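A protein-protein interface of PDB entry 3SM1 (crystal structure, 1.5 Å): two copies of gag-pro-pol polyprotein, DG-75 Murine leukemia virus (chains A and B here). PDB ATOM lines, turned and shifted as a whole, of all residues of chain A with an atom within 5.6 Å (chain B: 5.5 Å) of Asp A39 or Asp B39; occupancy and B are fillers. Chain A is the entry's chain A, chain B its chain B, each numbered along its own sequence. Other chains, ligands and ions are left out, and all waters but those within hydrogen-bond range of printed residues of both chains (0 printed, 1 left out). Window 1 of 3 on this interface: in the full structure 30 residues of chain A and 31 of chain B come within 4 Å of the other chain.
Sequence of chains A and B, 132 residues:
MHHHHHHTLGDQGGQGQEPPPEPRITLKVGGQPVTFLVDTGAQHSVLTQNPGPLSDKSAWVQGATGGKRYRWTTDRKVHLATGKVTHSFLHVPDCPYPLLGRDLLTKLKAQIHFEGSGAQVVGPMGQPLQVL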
ATOM      1  N   LEU A  37     -20.352 -27.324  14.876  1.00  0.00           N
ATOM      2  CA  LEU A  37     -19.701 -28.091  15.926  1.00  0.00           C
ATOM      3  C   LEU A  37     -20.277 -27.639  17.244  1.00  0.00           C
ATOM      4  O   LEU A  37     -20.297 -26.423  17.536  1.00  0.00           O
ATOM      5  CB  LEU A  37     -18.186 -27.811  15.896  1.00  0.00           C
ATOM      6  CG  LEU A  37     -17.331 -28.399  17.025  1.00  0.00           C
ATOM      7  CD1 LEU A  37     -17.433 -29.894  17.079  1.00  0.00           C
ATOM      8  CD2 LEU A  37     -15.881 -27.931  16.859  1.00  0.00           C
ATOM      9  N   VAL A  38     -20.715 -28.586  18.068  1.00  0.00           N
ATOM     10  CA  VAL A  38     -21.223 -28.254  19.391  1.00  0.00           C
ATOM     11  C   VAL A  38     -19.965 -28.043  20.248  1.00  0.00           C
ATOM     12  O   VAL A  38     -19.113 -28.941  20.346  1.00  0.00           O
ATOM     13  CB  VAL A  38     -22.118 -29.383  19.878  1.00  0.00           C
ATOM     14  CG1 VAL A  38     -22.508 -29.183  21.345  1.00  0.00           C
ATOM     15  CG2 VAL A  38     -23.327 -29.523  18.959  1.00  0.00           C
ATOM     16  N   ASP A  39     -19.821 -26.836  20.809  1.00  0.00           N
ATOM     17  CA  ASP A  39     -18.582 -26.428  21.469  1.00  0.00           C
ATOM     18  C   ASP A  39     -18.834 -25.864  22.841  1.00  0.00           C
ATOM     19  O   ASP A  39     -19.144 -24.653  22.999  1.00  0.00           O
ATOM     20  CB  ASP A  39     -17.890 -25.370  20.613  1.00  0.00           C
ATOM     21  CG  ASP A  39     -16.519 -25.014  21.120  1.00  0.00           C
ATOM     22  OD1 ASP A  39     -16.115 -25.508  22.189  1.00  0.00           O
ATOM     23  OD2 ASP A  39     -15.800 -24.248  20.436  1.00  0.00           O
ATOM     24  N   THR A  40     -18.704 -26.729  23.850  1.00  0.00           N
ATOM     25  CA  THR A  40     -19.010 -26.323  25.219  1.00  0.00           C
ATOM     26  C   THR A  40     -17.913 -25.377  25.738  1.00  0.00           C
ATOM     27  O   THR A  40     -18.116 -24.738  26.758  1.00  0.00           O
ATOM     28  CB  THR A  40     -19.136 -27.553  26.146  1.00  0.00           C
ATOM     29  OG1 THR A  40     -17.908 -28.297  26.099  1.00  0.00           O
ATOM     30  CG2 THR A  40     -20.280 -28.438  25.718  1.00  0.00           C
ATOM     31  N   GLY A  41     -16.790 -25.280  25.037  1.00  0.00           N
ATOM     32  CA  GLY A  41     -15.751 -24.302  25.393  1.00  0.00           C
ATOM     33  C   GLY A  41     -15.978 -22.906  24.805  1.00  0.00           C
ATOM     34  O   GLY A  41     -15.192 -21.973  25.099  1.00  0.00           O
ATOM     35  N   ALA A  42     -17.005 -22.731  23.982  1.00  0.00           N
ATOM     36  CA  ALA A  42     -17.303 -21.423  23.345  1.00  0.00           C
ATOM     37  C   ALA A  42     -18.379 -20.691  24.161  1.00  0.00           C
ATOM     38  O   ALA A  42     -19.473 -21.208  24.396  1.00  0.00           O
ATOM     39  CB  ALA A  42     -17.783 -21.632  21.922  1.00  0.00           C
ATOM     40  N   GLN A  43     -18.051 -19.493  24.644  1.00  0.00           N
ATOM     41  CA  GLN A  43     -18.987 -18.702  25.419  1.00  0.00           C
ATOM     42  C   GLN A  43     -20.168 -18.245  24.540  1.00  0.00           C
ATOM     43  O   GLN A  43     -21.288 -18.136  25.010  1.00  0.00           O
ATOM     44  CB  GLN A  43     -18.254 -17.489  25.993  1.00  0.00           C
ATOM     45  CG  GLN A  43     -19.065 -16.639  26.940  1.00  0.00           C
ATOM     46  CD  GLN A  43     -18.272 -15.468  27.460  1.00  0.00           C
ATOM     47  OE1 GLN A  43     -17.050 -15.451  27.399  1.00  0.00           O
ATOM     48  NE2 GLN A  43     -18.981 -14.478  27.991  1.00  0.00           N
ATOM     49  N   LEU A  99     -19.769 -22.609  15.296  1.00  0.00           N
ATOM     50  CA  LEU A  99     -19.759 -23.146  16.663  1.00  0.00           C
ATOM     51  C   LEU A  99     -21.060 -22.858  17.363  1.00  0.00           C
ATOM     52  O   LEU A  99     -21.536 -21.712  17.369  1.00  0.00           O
ATOM     53  CB  LEU A  99     -18.614 -22.533  17.503  1.00  0.00           C
ATOM     54  CG  LEU A  99     -17.219 -22.619  16.877  1.00  0.00           C
ATOM     55  CD1 LEU A  99     -16.260 -21.889  17.812  1.00  0.00           C
ATOM     56  CD2 LEU A  99     -16.735 -24.028  16.650  1.00  0.00           C
ATOM     57  N   LEU A 100     -21.625 -23.902  17.985  1.00  0.00           N
ATOM     58  CA  LEU A 100     -22.797 -23.742  18.821  1.00  0.00           C
ATOM     59  C   LEU A 100     -22.255 -23.767  20.243  1.00  0.00           C
ATOM     60  O   LEU A 100     -21.821 -24.820  20.766  1.00  0.00           O
ATOM     61  CB  LEU A 100     -23.821 -24.852  18.565  1.00  0.00           C
ATOM     62  CG  LEU A 100     -25.149 -24.563  19.241  1.00  0.00           C
ATOM     63  CD1 LEU A 100     -25.824 -23.471  18.427  1.00  0.00           C
ATOM     64  CD2 LEU A 100     -25.965 -25.824  19.184  1.00  0.00           C
ATOM     65  N   GLY A 101     -22.274 -22.587  20.862  1.00  0.00           N
ATOM     66  CA  GLY A 101     -21.677 -22.385  22.181  1.00  0.00           C
ATOM     67  C   GLY A 101     -22.658 -22.470  23.318  1.00  0.00           C
ATOM     68  O   GLY A 101     -23.809 -22.840  23.130  1.00  0.00           O
ATOM     69  N   ARG A 102     -22.167 -22.148  24.511  1.00  0.00           N
ATOM     70  CA  ARG A 102     -22.960 -22.337  25.722  1.00  0.00           C
ATOM     71  C   ARG A 102     -24.156 -21.403  25.758  1.00  0.00           C
ATOM     72  O   ARG A 102     -25.106 -21.702  26.472  1.00  0.00           O
ATOM     73  CB  ARG A 102     -22.100 -22.091  26.959  1.00  0.00           C
ATOM     74  CG  ARG A 102     -20.927 -23.050  27.080  1.00  0.00           C
ATOM     75  CD  ARG A 102     -20.274 -22.925  28.455  1.00  0.00           C
ATOM     76  NE  ARG A 102     -19.700 -21.597  28.734  1.00  0.00           N
ATOM     77  CZ  ARG A 102     -18.463 -21.222  28.400  1.00  0.00           C
ATOM     78  NH1 ARG A 102     -17.636 -22.018  27.738  1.00  0.00           N
ATOM     79  NH2 ARG A 102     -18.050 -19.997  28.717  1.00  0.00           N
ATOM     80  N   LEU A 105     -26.582 -23.612  23.842  1.00  0.00           N
ATOM     81  CA  LEU A 105     -26.755 -24.892  24.526  1.00  0.00           C
ATOM     82  C   LEU A 105     -27.608 -24.759  25.804  1.00  0.00           C
ATOM     83  O   LEU A 105     -28.377 -25.657  26.163  1.00  0.00           O
ATOM     84  CB  LEU A 105     -25.396 -25.513  24.867  1.00  0.00           C
ATOM     85  CG  LEU A 105     -24.607 -25.917  23.624  1.00  0.00           C
ATOM     86  CD1 LEU A 105     -23.122 -26.165  24.011  1.00  0.00           C
ATOM     87  CD2 LEU A 105     -25.221 -27.173  23.021  1.00  0.00           C
ATOM     88  N   LEU B  37     -11.779 -26.902  31.876  1.00  0.00           N
ATOM     89  CA  LEU B  37     -12.973 -26.611  31.130  1.00  0.00           C
ATOM     90  C   LEU B  37     -13.261 -27.792  30.222  1.00  0.00           C
ATOM     91  O   LEU B  37     -12.389 -28.236  29.440  1.00  0.00           O
ATOM     92  CB  LEU B  37     -12.776 -25.349  30.288  1.00  0.00           C
ATOM     93  CG  LEU B  37     -13.868 -24.965  29.307  1.00  0.00           C
ATOM     94  CD1 LEU B  37     -15.115 -24.662  30.072  1.00  0.00           C
ATOM     95  CD2 LEU B  37     -13.415 -23.738  28.495  1.00  0.00           C
ATOM     96  N   VAL B  38     -14.442 -28.358  30.332  1.00  0.00           N
ATOM     97  CA  VAL B  38     -14.804 -29.471  29.478  1.00  0.00           C
ATOM     98  C   VAL B  38     -15.167 -28.827  28.140  1.00  0.00           C
ATOM     99  O   VAL B  38     -16.085 -27.978  28.034  1.00  0.00           O
ATOM    100  CB  VAL B  38     -15.943 -30.241  30.117  1.00  0.00           C
ATOM    101  CG1 VAL B  38     -16.505 -31.254  29.137  1.00  0.00           C
ATOM    102  CG2 VAL B  38     -15.397 -30.962  31.333  1.00  0.00           C
ATOM    103  N   ASP B  39     -14.432 -29.222  27.097  1.00  0.00           N
ATOM    104  CA  ASP B  39     -14.501 -28.522  25.835  1.00  0.00           C
ATOM    105  C   ASP B  39     -14.738 -29.481  24.662  1.00  0.00           C
ATOM    106  O   ASP B  39     -13.786 -30.060  24.100  1.00  0.00           O
ATOM    107  CB  ASP B  39     -13.209 -27.740  25.634  1.00  0.00           C
ATOM    108  CG  ASP B  39     -13.263 -26.864  24.414  1.00  0.00           C
ATOM    109  OD1 ASP B  39     -14.301 -26.889  23.716  1.00  0.00           O
ATOM    110  OD2 ASP B  39     -12.280 -26.132  24.186  1.00  0.00           O
ATOM    111  N   THR B  40     -15.992 -29.620  24.261  1.00  0.00           N
ATOM    112  CA  THR B  40     -16.302 -30.504  23.141  1.00  0.00           C
ATOM    113  C   THR B  40     -15.753 -29.991  21.821  1.00  0.00           C
ATOM    114  O   THR B  40     -15.696 -30.754  20.864  1.00  0.00           O
ATOM    115  CB  THR B  40     -17.808 -30.792  23.042  1.00  0.00           C
ATOM    116  OG1 THR B  40     -18.490 -29.544  22.906  1.00  0.00           O
ATOM    117  CG2 THR B  40     -18.286 -31.468  24.327  1.00  0.00           C
ATOM    118  N   GLY B  41     -15.360 -28.723  21.779  1.00  0.00           N
ATOM    119  CA  GLY B  41     -14.743 -28.132  20.594  1.00  0.00           C
ATOM    120  C   GLY B  41     -13.272 -28.408  20.477  1.00  0.00           C
ATOM    121  O   GLY B  41     -12.672 -28.042  19.471  1.00  0.00           O
ATOM    122  N   ALA B  42     -12.671 -29.031  21.493  1.00  0.00           N
ATOM    123  CA  ALA B  42     -11.235 -29.331  21.465  1.00  0.00           C
ATOM    124  C   ALA B  42     -10.987 -30.778  20.998  1.00  0.00           C
ATOM    125  O   ALA B  42     -11.445 -31.754  21.594  1.00  0.00           O
ATOM    126  CB  ALA B  42     -10.600 -29.095  22.857  1.00  0.00           C
ATOM    127  N   LEU B  99      -7.996 -27.560  29.018  1.00  0.00           N
ATOM    128  CA  LEU B  99      -9.196 -28.023  28.292  1.00  0.00           C
ATOM    129  C   LEU B  99      -9.218 -29.541  28.298  1.00  0.00           C
ATOM    130  O   LEU B  99      -8.221 -30.206  27.965  1.00  0.00           O
ATOM    131  CB  LEU B  99      -9.171 -27.552  26.844  1.00  0.00           C
ATOM    132  CG  LEU B  99      -8.915 -26.085  26.599  1.00  0.00           C
ATOM    133  CD1 LEU B  99      -8.820 -25.827  25.090  1.00  0.00           C
ATOM    134  CD2 LEU B  99     -10.001 -25.215  27.240  1.00  0.00           C
ATOM    135  N   LEU B 100     -10.372 -30.116  28.640  1.00  0.00           N
ATOM    136  CA  LEU B 100     -10.567 -31.541  28.540  1.00  0.00           C
ATOM    137  C   LEU B 100     -11.394 -31.740  27.282  1.00  0.00           C
ATOM    138  O   LEU B 100     -12.569 -31.362  27.210  1.00  0.00           O
ATOM    139  CB  LEU B 100     -11.304 -32.072  29.779  1.00  0.00           C
ATOM    140  CG  LEU B 100     -11.251 -33.597  29.903  1.00  0.00           C
ATOM    141  CD1 LEU B 100     -11.460 -34.029  31.334  1.00  0.00           C
ATOM    142  CD2 LEU B 100     -12.336 -34.158  29.067  1.00  0.00           C
ATOM    143  N   GLY B 101     -10.744 -32.294  26.264  1.00  0.00           N
ATOM    144  CA  GLY B 101     -11.307 -32.348  24.924  1.00  0.00           C
ATOM    145  C   GLY B 101     -11.916 -33.698  24.595  1.00  0.00           C
ATOM    146  O   GLY B 101     -12.091 -34.571  25.462  1.00  0.00           O
ATOM    147  N   ARG B 102     -12.230 -33.853  23.320  1.00  0.00           N
ATOM    148  CA  ARG B 102     -12.979 -35.052  22.864  1.00  0.00           C
ATOM    149  C   ARG B 102     -12.172 -36.324  23.031  1.00  0.00           C
ATOM    150  O   ARG B 102     -12.760 -37.407  23.132  1.00  0.00           O
ATOM    151  CB  ARG B 102     -13.388 -34.879  21.412  1.00  0.00           C
ATOM    152  CG  ARG B 102     -14.316 -33.674  21.179  1.00  0.00           C
ATOM    153  CD  ARG B 102     -14.965 -33.717  19.777  1.00  0.00           C
ATOM    154  NE  ARG B 102     -13.954 -33.610  18.723  1.00  0.00           N
ATOM    155  CZ  ARG B 102     -13.479 -32.468  18.236  1.00  0.00           C
ATOM    156  NH1 ARG B 102     -13.895 -31.276  18.688  1.00  0.00           N
ATOM    157  NH2 ARG B 102     -12.576 -32.498  17.257  1.00  0.00           N
ATOM    158  N   LEU B 105     -12.931 -37.132  26.719  1.00  0.00           N
ATOM    159  CA  LEU B 105     -14.375 -37.310  26.885  1.00  0.00           C
ATOM    160  C   LEU B 105     -14.805 -38.678  26.358  1.00  0.00           C
ATOM    161  O   LEU B 105     -15.690 -39.322  26.960  1.00  0.00           O
ATOM    162  CB  LEU B 105     -15.167 -36.191  26.231  1.00  0.00           C
ATOM    163  CG  LEU B 105     -15.019 -34.833  26.921  1.00  0.00           C
ATOM    164  CD1 LEU B 105     -15.507 -33.664  26.075  1.00  0.00           C
ATOM    165  CD2 LEU B 105     -15.747 -34.846  28.270  1.00  0.00           C
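Hydrophobic or aromatic side chains of chain A that line the printed part of chain B: Leu A37. Along chain A the printed residues that touch a printed residue of chain B span positions 37 to 41. Printed residues of chain B that touch a printed residue of chain A: Leu B37, Val B38, Asp B39, Thr B40 and Gly B41. Hydrophobic or aromatic side chains of chain B within 4 Å of the printed part of chain A: Leu B37.
Leu A37 touches Gly B41. Thr B40 touches Asp A39. OG1 of Thr A40 touches CA of Asp B39, 3.4 Å away. Leu B37 touches Gly A41 (CD2 to CA, 3.9 Å).
The backbone NH (N) of Leu A100 lies within hydrogen-bond range of the backbone carbonyl oxygen (O) of Leu A37 (2.9 Å). N of Gly A41 sits at hydrogen-bond distance from OD1 of Asp A39, 2.9 Å away. The side-chain carboxylate (OD1) of Asp B39 sits at hydrogen-bond distance from the backbone NH (N) of Gly B41 (2.9 Å). The side-chain carboxylate (OD1) of Asp B39 is in hydrogen-bond range of the backbone NH (N) of Ala B42 (3.5 Å). N of Asp B39 sits at hydrogen-bond distance from O of Leu B100 (2.8 Å). The backbone carbonyl oxygen (O) of Thr B40 is in hydrogen-bond range of the guanidinium group (NH1) of Arg B102, 2.9 Å away.
The backbone carbonyl oxygen (O) of Val A38 sits at hydrogen-bond distance from the side-chain hydroxyl (OG1) of Thr B40, at 2.7 Å. The side-chain carboxylate (OD1) of Asp A39 lies close to the side-chain carboxylate (OD1) of Asp B39 (2.7 Å). N of Gly B41 sits at hydrogen-bond distance from OD1 of Asp A39 (3.3 Å). The side-chain hydroxyl (OG1) of Thr A40 lies within hydrogen-bond range of the backbone carbonyl oxygen (O) of Val B38 (2.7 Å). The backbone NH of Thr B40 lies within hydrogen-bond range of the side-chain hydroxyl of Thr A40 (3.0 Å). The backbone NH (N) of Gly A41 is in hydrogen-bond range of the side-chain carboxylate (OD1) of Asp B39, 3.2 Å away.
Of chain B, only Asp B39, Thr B40 and Gly B41 come within 4 Å of Asp A39. Of the printed residues of chain B, Thr A40 touches Val B38, Asp B39 and Thr B40. Printed residues of chain B within 4 Å of Gly A41: Leu B37 (3.9 Å) and Asp B39 (3.2 Å). Of the printed residues of chain A, Leu B37 touches Gly A41. Of the printed residues of chain A, Val B38 touches Thr A40. Asp B39 touches three residues of chain A. The nearest residue of chain B that does not touch Asp A39 is Ala B42 (5.0 Å). The nearest residue of chain A that does not touch Asp B39 is Ala A42 (5.0 Å). The nearest printed residue of chain B that does not touch Val A38 is Gly B41 (4.02 Å).
Leu A37 touches Gly B41, and with the chains exchanged Gly A41 touches Leu B37. Asp B39 touches its own counterpart, Asp A39. Asp A39 touches Gly B41, and with the chains exchanged Gly A41 touches Asp B39. Thr B40 touches its own counterpart, Thr A40.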
